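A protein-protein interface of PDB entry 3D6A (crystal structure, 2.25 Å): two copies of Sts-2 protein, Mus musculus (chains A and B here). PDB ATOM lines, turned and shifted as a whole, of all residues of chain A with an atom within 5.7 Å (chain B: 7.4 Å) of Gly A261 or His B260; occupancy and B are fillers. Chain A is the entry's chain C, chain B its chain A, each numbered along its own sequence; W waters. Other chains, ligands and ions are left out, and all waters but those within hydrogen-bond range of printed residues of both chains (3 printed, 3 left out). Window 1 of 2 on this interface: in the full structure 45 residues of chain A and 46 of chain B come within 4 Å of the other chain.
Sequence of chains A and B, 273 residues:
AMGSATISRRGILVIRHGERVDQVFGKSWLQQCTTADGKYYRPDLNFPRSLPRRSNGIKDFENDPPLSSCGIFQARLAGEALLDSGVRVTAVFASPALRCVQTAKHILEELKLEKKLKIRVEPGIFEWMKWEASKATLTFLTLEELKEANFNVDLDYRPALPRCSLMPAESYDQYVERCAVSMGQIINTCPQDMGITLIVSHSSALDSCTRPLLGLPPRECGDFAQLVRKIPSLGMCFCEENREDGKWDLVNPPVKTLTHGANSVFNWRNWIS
The backbone carbonyl oxygen of Leu B258 is in hydrogen-bond range of the side-chain amide nitrogen of Asn A263, at 2.9 Å. O of Thr B259 is in hydrogen-bond range of ND2 of Asn A46 (2.8 Å). N of Asn A263 is in hydrogen-bond range of O of His B260, at 2.9 Å. ND2 of Asn B46 is in hydrogen-bond range of O of Thr A259. The backbone carbonyl oxygen (O) of His A260 is in hydrogen-bond range of the backbone NH (N) of Asn B263, at 2.9 Å. OD1 of Asn A263 lies within hydrogen-bond range of N of Ser B233 (3.1 Å). OE2 of Glu B19 sits at hydrogen-bond distance from N of Gly A261, at 2.9 Å. A ring nitrogen (ND1) of His B260 is in hydrogen-bond range of the side-chain sulfur (SG) of Cys A70, at 3.7 Å. The backbone NH of Gly B261 lies within hydrogen-bond range of the side-chain carboxylate of Glu A19. OD2 of Asp A44 is in hydrogen-bond range of OG1 of Thr B259 (2.7 Å).
N of Cys B70 sits at hydrogen-bond distance from OD1 of Asn B46 (2.9 Å). The side-chain carboxylate of Asp A44 lies within hydrogen-bond range of the backbone NH of Asn A46. SG of Cys B70 sits at hydrogen-bond distance from NE2 of Gln B74, 3.8 Å away. N of Cys B70 lies close to OG of Ser B68 (3.4 Å). NE2 of Gln B74 is in hydrogen-bond range of NE2 of His B260 (3.0 Å). The side-chain carboxylate (OE1) of Glu B19 lies within hydrogen-bond range of the side-chain amide nitrogen (ND2) of Asn B46, 2.9 Å away.
CG1 of Val A24 touches O of Thr B259, at 3.8 Å. N of Gly B261 touches CG2 of Val A24 (3.8 Å). Asp A44 touches Leu B258 (OD1 to CA, 3.5 Å). Cys A70 touches Phe B73 (CA to CZ, 3.6 Å). His A260 touches Cys B70. Gly B261 touches His A260. His A260 touches Ala B262. Gly A261 touches Gly B261 (O to O, 3.5 Å). Ala A262 touches Gly B261 (CA to C, 3.8 Å). Ala B262 touches Ala A262 (CB to N, 3.8 Å).
Gly A261 touches just these residues of chain B: Glu B19 (2.9 Å), His B260 (3.1 Å), Gly B261 (3.5 Å) and Ala B262 (3.7 Å). Printed residues of chain A within 4 Å of His B260: Glu A19, Asn A46, Cys A70, Gly A261, Ala A262 and Asn A263. Of the printed residues of chain B, Asn A263 touches Gln B74 (3.9 Å), Ser B233 (3.1 Å), Leu B258 (2.9 Å), Thr B259 (3.5 Å) and His B260 (2.9 Å). Of the printed residues of chain B, Thr A259 touches Val B24 (3.6 Å), Asn B46 (2.9 Å) and Asn B263 (3.3 Å). Of the printed residues of chain B, Cys A70 touches Phe B73 (3.6 Å) and His B260 (3.7 Å). Printed residues of chain B within 4 Å of Val A24: Thr B259 (3.8 Å) and Gly B261 (3.8 Å). Of the printed residues of chain A, Glu B19 touches His A260 and Gly A261. Ser B68 touches none of the printed residues of chain A. The nearest residue of chain A that does not touch His B260 is His A260 (4.2 Å). The nearest printed residue of chain B that does not touch Thr A259 is Ser B264 (4.3 Å).
Hydrophobic or aromatic side chains of chain A within 4 Å of the printed part of chain B: Val A24, His A260 and Ala A262. Along chain A the printed residues that touch a printed residue of chain B span positions 19 to 263. Of the 18 printed residues of chain B, 13 touch a printed residue of chain A. Among the printed residues, 32 pairs touch across the chains. Among the printed residues, no Asp or Glu carboxylate lies within 4 Å of a Lys or Arg side-chain nitrogen of the other chain.
Glu A19 touches Gly B261, and with the chains exchanged Gly A261 touches Glu B19. Asn A46 touches His B260, and with the chains exchanged His A260 touches Asn B46. Cys A70 touches His B260, and with the chains exchanged His A260 touches Cys B70. Gly A261 touches Ala B262, and with the chains exchanged Ala A262 touches Gly B261. Positions printed for both chains: 19, 24, 46, 70, 259, 260, 261, 262, 263 and 264. Of the 32 pairs that touch across the chains among the printed residues, 24 have their exchanged pair printed and touching as well.
Water W3 lies within hydrogen-bond range of the backbone carbonyl oxygen of Ser A264 (2.7 Å) and the backbone carbonyl oxygen of Leu B258 (3.0 Å). Water W1 bridges O of Ser B233 (2.7 Å) and ND2 of Asn A263 (3.3 Å). Water W2 bridges the backbone carbonyl oxygen of Asn B263 (2.8 Å) and the backbone carbonyl oxygen of His A260 (3.1 Å).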
ATOM      1  N   GLU A  19      13.738 -14.459 -14.346  1.00  0.00           N
ATOM      2  CA  GLU A  19      12.942 -14.788 -15.524  1.00  0.00           C
ATOM      3  C   GLU A  19      11.755 -15.684 -15.189  1.00  0.00           C
ATOM      4  O   GLU A  19      11.897 -16.690 -14.460  1.00  0.00           O
ATOM      5  CB  GLU A  19      13.828 -15.465 -16.582  1.00  0.00           C
ATOM      6  CG  GLU A  19      13.111 -15.801 -17.902  1.00  0.00           C
ATOM      7  CD  GLU A  19      13.973 -16.614 -18.840  1.00  0.00           C
ATOM      8  OE1 GLU A  19      14.098 -17.840 -18.659  1.00  0.00           O
ATOM      9  OE2 GLU A  19      14.550 -16.032 -19.775  1.00  0.00           O
ATOM     10  N   VAL A  24       9.010 -16.393 -21.613  1.00  0.00           N
ATOM     11  CA  VAL A  24       9.667 -17.199 -22.639  1.00  0.00           C
ATOM     12  C   VAL A  24       8.648 -17.993 -23.453  1.00  0.00           C
ATOM     13  O   VAL A  24       8.749 -18.060 -24.661  1.00  0.00           O
ATOM     14  CB  VAL A  24      10.714 -18.179 -22.045  1.00  0.00           C
ATOM     15  CG1 VAL A  24      11.245 -19.125 -23.123  1.00  0.00           C
ATOM     16  CG2 VAL A  24      11.872 -17.425 -21.385  1.00  0.00           C
ATOM     17  N   ASP A  44      10.103 -28.605 -21.919  1.00  0.00           N
ATOM     18  CA  ASP A  44      11.354 -27.924 -22.235  1.00  0.00           C
ATOM     19  C   ASP A  44      12.008 -27.773 -20.866  1.00  0.00           C
ATOM     20  O   ASP A  44      11.302 -27.630 -19.853  1.00  0.00           O
ATOM     21  CB  ASP A  44      11.055 -26.557 -22.875  1.00  0.00           C
ATOM     22  CG  ASP A  44      12.337 -25.781 -23.315  1.00  0.00           C
ATOM     23  OD1 ASP A  44      13.030 -25.164 -22.467  1.00  0.00           O
ATOM     24  OD2 ASP A  44      12.621 -25.757 -24.531  1.00  0.00           O
ATOM     25  N   ASN A  46      13.517 -25.371 -19.490  1.00  0.00           N
ATOM     26  CA  ASN A  46      13.285 -24.072 -18.856  1.00  0.00           C
ATOM     27  C   ASN A  46      11.989 -23.997 -18.034  1.00  0.00           C
ATOM     28  O   ASN A  46      11.828 -23.103 -17.198  1.00  0.00           O
ATOM     29  CB  ASN A  46      13.372 -22.926 -19.866  1.00  0.00           C
ATOM     30  CG  ASN A  46      13.852 -21.626 -19.240  1.00  0.00           C
ATOM     31  OD1 ASN A  46      14.649 -21.625 -18.295  1.00  0.00           O
ATOM     32  ND2 ASN A  46      13.380 -20.508 -19.775  1.00  0.00           N
ATOM     33  N   CYS A  70      15.994 -20.824 -15.854  1.00  0.00           N
ATOM     34  CA  CYS A  70      16.955 -19.742 -16.027  1.00  0.00           C
ATOM     35  C   CYS A  70      16.761 -18.694 -14.929  1.00  0.00           C
ATOM     36  O   CYS A  70      17.733 -18.255 -14.353  1.00  0.00           O
ATOM     37  CB  CYS A  70      16.835 -19.149 -17.438  1.00  0.00           C
ATOM     38  SG  CYS A  70      18.163 -18.014 -17.869  1.00  0.00           S
ATOM     39  N   THR A 259      25.000 -10.286 -17.448  1.00  0.00           N
ATOM     40  CA  THR A 259      24.714 -10.291 -18.885  1.00  0.00           C
ATOM     41  C   THR A 259      24.847 -11.714 -19.420  1.00  0.00           C
ATOM     42  O   THR A 259      25.887 -12.333 -19.243  1.00  0.00           O
ATOM     43  CB  THR A 259      25.764  -9.428 -19.685  1.00  0.00           C
ATOM     44  OG1 THR A 259      26.069  -8.234 -18.967  1.00  0.00           O
ATOM     45  CG2 THR A 259      25.241  -9.057 -21.070  1.00  0.00           C
ATOM     46  N   HIS A 260      23.820 -12.236 -20.071  1.00  0.00           N
ATOM     47  CA  HIS A 260      23.970 -13.509 -20.783  1.00  0.00           C
ATOM     48  C   HIS A 260      23.068 -13.525 -22.018  1.00  0.00           C
ATOM     49  O   HIS A 260      22.182 -12.689 -22.125  1.00  0.00           O
ATOM     50  CB  HIS A 260      23.755 -14.751 -19.872  1.00  0.00           C
ATOM     51  CG  HIS A 260      22.393 -14.847 -19.256  1.00  0.00           C
ATOM     52  ND1 HIS A 260      21.272 -15.211 -19.971  1.00  0.00           N
ATOM     53  CD2 HIS A 260      21.976 -14.650 -17.981  1.00  0.00           C
ATOM     54  CE1 HIS A 260      20.226 -15.239 -19.167  1.00  0.00           C
ATOM     55  NE2 HIS A 260      20.627 -14.898 -17.955  1.00  0.00           N
ATOM     56  N   GLY A 261      23.332 -14.439 -22.948  1.00  0.00           N
ATOM     57  CA  GLY A 261      22.538 -14.553 -24.164  1.00  0.00           C
ATOM     58  C   GLY A 261      21.379 -15.525 -23.978  1.00  0.00           C
ATOM     59  O   GLY A 261      21.215 -16.167 -22.908  1.00  0.00           O
ATOM     60  N   ALA A 262      20.575 -15.597 -25.028  1.00  0.00           N
ATOM     61  CA  ALA A 262      19.416 -16.460 -25.124  1.00  0.00           C
ATOM     62  C   ALA A 262      19.826 -17.862 -25.573  1.00  0.00           C
ATOM     63  O   ALA A 262      20.941 -18.096 -26.003  1.00  0.00           O
ATOM     64  CB  ALA A 262      18.409 -15.852 -26.152  1.00  0.00           C
ATOM     65  N   ASN A 263      18.904 -18.805 -25.469  1.00  0.00           N
ATOM     66  CA  ASN A 263      19.069 -20.095 -26.105  1.00  0.00           C
ATOM     67  C   ASN A 263      17.802 -20.299 -26.911  1.00  0.00           C
ATOM     68  O   ASN A 263      16.717 -20.300 -26.361  1.00  0.00           O
ATOM     69  CB  ASN A 263      19.202 -21.182 -25.047  1.00  0.00           C
ATOM     70  CG  ASN A 263      20.197 -22.225 -25.414  1.00  0.00           C
ATOM     71  OD1 ASN A 263      21.252 -21.914 -25.944  1.00  0.00           O
ATOM     72  ND2 ASN A 263      19.886 -23.474 -25.125  1.00  0.00           N
ATOM     73  N   SER A 264      17.951 -20.428 -28.224  1.00  0.00           N
ATOM     74  CA  SER A 264      16.816 -20.446 -29.133  1.00  0.00           C
ATOM     75  C   SER A 264      16.172 -21.810 -29.213  1.00  0.00           C
ATOM     76  O   SER A 264      16.822 -22.806 -28.984  1.00  0.00           O
ATOM     77  CB  SER A 264      17.254 -20.025 -30.547  1.00  0.00           C
ATOM     78  OG  SER A 264      17.283 -18.613 -30.664  1.00  0.00           O
ATOM     79  N   GLU B  19      27.254 -22.079 -23.181  1.00  0.00           N
ATOM     80  CA  GLU B  19      27.603 -20.722 -23.542  1.00  0.00           C
ATOM     81  C   GLU B  19      29.036 -20.429 -23.093  1.00  0.00           C
ATOM     82  O   GLU B  19      29.383 -20.661 -21.936  1.00  0.00           O
ATOM     83  CB  GLU B  19      26.624 -19.738 -22.862  1.00  0.00           C
ATOM     84  CG  GLU B  19      26.824 -18.286 -23.260  1.00  0.00           C
ATOM     85  CD  GLU B  19      25.996 -17.325 -22.434  1.00  0.00           C
ATOM     86  OE1 GLU B  19      26.334 -17.096 -21.240  1.00  0.00           O
ATOM     87  OE2 GLU B  19      25.011 -16.783 -22.986  1.00  0.00           O
ATOM     88  N   GLN B  23      31.289 -15.513 -26.433  1.00  0.00           N
ATOM     89  CA  GLN B  23      29.993 -15.305 -27.123  1.00  0.00           C
ATOM     90  C   GLN B  23      29.285 -14.065 -26.574  1.00  0.00           C
ATOM     91  O   GLN B  23      28.609 -13.343 -27.315  1.00  0.00           O
ATOM     92  CB  GLN B  23      29.033 -16.484 -26.913  1.00  0.00           C
ATOM     93  CG  GLN B  23      29.433 -17.809 -27.531  1.00  0.00           C
ATOM     94  CD  GLN B  23      28.365 -18.911 -27.310  1.00  0.00           C
ATOM     95  OE1 GLN B  23      28.659 -20.005 -26.791  1.00  0.00           O
ATOM     96  NE2 GLN B  23      27.116 -18.610 -27.709  1.00  0.00           N
ATOM     97  N   VAL B  24      29.413 -13.838 -25.267  1.00  0.00           N
ATOM     98  CA  VAL B  24      28.713 -12.729 -24.608  1.00  0.00           C
ATOM     99  C   VAL B  24      29.556 -11.462 -24.565  1.00  0.00           C
ATOM    100  O   VAL B  24      29.084 -10.396 -24.907  1.00  0.00           O
ATOM    101  CB  VAL B  24      28.220 -13.098 -23.157  1.00  0.00           C
ATOM    102  CG1 VAL B  24      27.426 -11.933 -22.526  1.00  0.00           C
ATOM    103  CG2 VAL B  24      27.358 -14.346 -23.198  1.00  0.00           C
ATOM    104  N   ASN B  46      28.388 -13.120 -15.163  1.00  0.00           N
ATOM    105  CA  ASN B  46      28.453 -14.174 -16.163  1.00  0.00           C
ATOM    106  C   ASN B  46      29.885 -14.678 -16.448  1.00  0.00           C
ATOM    107  O   ASN B  46      30.092 -15.700 -17.097  1.00  0.00           O
ATOM    108  CB  ASN B  46      27.698 -13.783 -17.423  1.00  0.00           C
ATOM    109  CG  ASN B  46      27.260 -15.003 -18.244  1.00  0.00           C
ATOM    110  OD1 ASN B  46      26.922 -16.062 -17.688  1.00  0.00           O
ATOM    111  ND2 ASN B  46      27.264 -14.854 -19.572  1.00  0.00           N
ATOM    112  N   SER B  68      30.757 -19.526 -19.627  1.00  0.00           N
ATOM    113  CA  SER B  68      30.225 -18.474 -18.798  1.00  0.00           C
ATOM    114  C   SER B  68      29.468 -19.136 -17.624  1.00  0.00           C
ATOM    115  O   SER B  68      29.296 -20.351 -17.605  1.00  0.00           O
ATOM    116  CB  SER B  68      29.321 -17.583 -19.660  1.00  0.00           C
ATOM    117  OG  SER B  68      28.127 -18.270 -19.995  1.00  0.00           O
ATOM    118  N   CYS B  70      26.324 -18.830 -17.214  1.00  0.00           N
ATOM    119  CA  CYS B  70      25.104 -19.326 -17.864  1.00  0.00           C
ATOM    120  C   CYS B  70      25.366 -20.670 -18.538  1.00  0.00           C
ATOM    121  O   CYS B  70      24.527 -21.564 -18.488  1.00  0.00           O
ATOM    122  CB  CYS B  70      24.550 -18.306 -18.873  1.00  0.00           C
ATOM    123  SG  CYS B  70      22.937 -18.734 -19.551  1.00  0.00           S
ATOM    124  N   GLY B  71      26.541 -20.829 -19.129  1.00  0.00           N
ATOM    125  CA  GLY B  71      26.898 -22.084 -19.807  1.00  0.00           C
ATOM    126  C   GLY B  71      27.063 -23.254 -18.849  1.00  0.00           C
ATOM    127  O   GLY B  71      26.798 -24.379 -19.221  1.00  0.00           O
ATOM    128  N   PHE B  73      25.358 -23.407 -15.905  1.00  0.00           N
ATOM    129  CA  PHE B  73      23.931 -23.657 -15.650  1.00  0.00           C
ATOM    130  C   PHE B  73      23.291 -24.570 -16.717  1.00  0.00           C
ATOM    131  O   PHE B  73      22.620 -25.557 -16.387  1.00  0.00           O
ATOM    132  CB  PHE B  73      23.167 -22.322 -15.504  1.00  0.00           C
ATOM    133  CG  PHE B  73      21.734 -22.358 -16.018  1.00  0.00           C
ATOM    134  CD1 PHE B  73      20.745 -23.082 -15.334  1.00  0.00           C
ATOM    135  CD2 PHE B  73      21.384 -21.653 -17.172  1.00  0.00           C
ATOM    136  CE1 PHE B  73      19.451 -23.122 -15.799  1.00  0.00           C
ATOM    137  CE2 PHE B  73      20.093 -21.687 -17.666  1.00  0.00           C
ATOM    138  CZ  PHE B  73      19.110 -22.434 -16.981  1.00  0.00           C
ATOM    139  N   GLN B  74      23.495 -24.235 -17.988  1.00  0.00           N
ATOM    140  CA  GLN B  74      22.951 -25.046 -19.073  1.00  0.00           C
ATOM    141  C   GLN B  74      23.453 -26.496 -18.993  1.00  0.00           C
ATOM    142  O   GLN B  74      22.671 -27.436 -19.106  1.00  0.00           O
ATOM    143  CB  GLN B  74      23.295 -24.428 -20.432  1.00  0.00           C
ATOM    144  CG  GLN B  74      22.697 -23.023 -20.630  1.00  0.00           C
ATOM    145  CD  GLN B  74      23.370 -22.262 -21.763  1.00  0.00           C
ATOM    146  OE1 GLN B  74      24.535 -22.511 -22.101  1.00  0.00           O
ATOM    147  NE2 GLN B  74      22.656 -21.313 -22.327  1.00  0.00           N
ATOM    148  N   LEU B  77      21.945 -28.221 -15.993  1.00  0.00           N
ATOM    149  CA  LEU B  77      20.520 -28.459 -16.175  1.00  0.00           C
ATOM    150  C   LEU B  77      20.265 -29.693 -17.066  1.00  0.00           C
ATOM    151  O   LEU B  77      19.326 -30.466 -16.825  1.00  0.00           O
ATOM    152  CB  LEU B  77      19.859 -27.227 -16.781  1.00  0.00           C
ATOM    153  CG  LEU B  77      18.335 -27.269 -16.791  1.00  0.00           C
ATOM    154  CD1 LEU B  77      17.820 -27.116 -15.345  1.00  0.00           C
ATOM    155  CD2 LEU B  77      17.857 -26.149 -17.697  1.00  0.00           C
ATOM    156  N   SER B 233      23.245 -23.708 -27.427  1.00  0.00           N
ATOM    157  CA  SER B 233      24.076 -24.218 -26.344  1.00  0.00           C
ATOM    158  C   SER B 233      23.428 -25.469 -25.797  1.00  0.00           C
ATOM    159  O   SER B 233      22.214 -25.483 -25.575  1.00  0.00           O
ATOM    160  CB  SER B 233      24.190 -23.172 -25.233  1.00  0.00           C
ATOM    161  OG  SER B 233      24.905 -22.044 -25.694  1.00  0.00           O
ATOM    162  N   LEU B 258      16.268 -26.798 -24.349  1.00  0.00           N
ATOM    163  CA  LEU B 258      16.341 -25.746 -23.367  1.00  0.00           C
ATOM    164  C   LEU B 258      16.183 -24.412 -24.059  1.00  0.00           C
ATOM    165  O   LEU B 258      17.040 -24.000 -24.815  1.00  0.00           O
ATOM    166  CB  LEU B 258      17.679 -25.791 -22.598  1.00  0.00           C
ATOM    167  CG  LEU B 258      17.994 -24.522 -21.768  1.00  0.00           C
ATOM    168  CD1 LEU B 258      16.933 -24.228 -20.702  1.00  0.00           C
ATOM    169  CD2 LEU B 258      19.389 -24.594 -21.143  1.00  0.00           C
ATOM    170  N   THR B 259      15.094 -23.722 -23.765  1.00  0.00           N
ATOM    171  CA  THR B 259      14.825 -22.440 -24.372  1.00  0.00           C
ATOM    172  C   THR B 259      14.782 -21.417 -23.271  1.00  0.00           C
ATOM    173  O   THR B 259      14.011 -21.577 -22.335  1.00  0.00           O
ATOM    174  CB  THR B 259      13.451 -22.438 -25.062  1.00  0.00           C
ATOM    175  OG1 THR B 259      13.379 -23.549 -25.955  1.00  0.00           O
ATOM    176  CG2 THR B 259      13.235 -21.133 -25.828  1.00  0.00           C
ATOM    177  N   HIS B 260      15.585 -20.360 -23.397  1.00  0.00           N
ATOM    178  CA  HIS B 260      15.559 -19.266 -22.420  1.00  0.00           C
ATOM    179  C   HIS B 260      15.918 -17.916 -23.022  1.00  0.00           C
ATOM    180  O   HIS B 260      16.517 -17.848 -24.085  1.00  0.00           O
ATOM    181  CB  HIS B 260      16.409 -19.583 -21.172  1.00  0.00           C
ATOM    182  CG  HIS B 260      17.892 -19.592 -21.408  1.00  0.00           C
ATOM    183  ND1 HIS B 260      18.641 -18.440 -21.512  1.00  0.00           N
ATOM    184  CD2 HIS B 260      18.768 -20.616 -21.528  1.00  0.00           C
ATOM    185  CE1 HIS B 260      19.909 -18.749 -21.714  1.00  0.00           C
ATOM    186  NE2 HIS B 260      20.013 -20.064 -21.716  1.00  0.00           N
ATOM    187  N   GLY B 261      15.542 -16.843 -22.336  1.00  0.00           N
ATOM    188  CA  GLY B 261      15.805 -15.488 -22.799  1.00  0.00           C
ATOM    189  C   GLY B 261      17.198 -15.022 -22.437  1.00  0.00           C
ATOM    190  O   GLY B 261      17.939 -15.714 -21.719  1.00  0.00           O
ATOM    191  N   ALA B 262      17.550 -13.859 -22.975  1.00  0.00           N
ATOM    192  CA  ALA B 262      18.785 -13.169 -22.665  1.00  0.00           C
ATOM    193  C   ALA B 262      18.622 -12.319 -21.398  1.00  0.00           C
ATOM    194  O   ALA B 262      17.509 -12.098 -20.910  1.00  0.00           O
ATOM    195  CB  ALA B 262      19.207 -12.282 -23.861  1.00  0.00           C
ATOM    196  N   ASN B 263      19.743 -11.860 -20.863  1.00  0.00           N
ATOM    197  CA  ASN B 263      19.733 -10.870 -19.816  1.00  0.00           C
ATOM    198  C   ASN B 263      20.671  -9.748 -20.237  1.00  0.00           C
ATOM    199  O   ASN B 263      21.858  -9.982 -20.455  1.00  0.00           O
ATOM    200  CB  ASN B 263      20.155 -11.459 -18.472  1.00  0.00           C
ATOM    201  CG  ASN B 263      19.424 -10.805 -17.312  1.00  0.00           C
ATOM    202  OD1 ASN B 263      20.042 -10.203 -16.439  1.00  0.00           O
ATOM    203  ND2 ASN B 263      18.094 -10.864 -17.339  1.00  0.00           N
ATOM    204  N   SER B 264      20.131  -8.542 -20.374  1.00  0.00           N
ATOM    205  CA  SER B 264      20.926  -7.436 -20.905  1.00  0.00           C
ATOM    206  C   SER B 264      21.789  -6.803 -19.834  1.00  0.00           C
ATOM    207  O   SER B 264      21.483  -6.896 -18.639  1.00  0.00           O
ATOM    208  CB  SER B 264      20.035  -6.390 -21.562  1.00  0.00           C
ATOM    209  OG  SER B 264      19.046  -5.945 -20.645  1.00  0.00           O
HETATM  210  O   HOH W   1      19.852 -26.772 -25.230  1.00  0.00           O
HETATM  211  O   HOH W   2      22.569  -9.824 -23.184  1.00  0.00           O
HETATM  212  O   HOH W   3      16.837 -25.109 -27.636  1.00  0.00           O
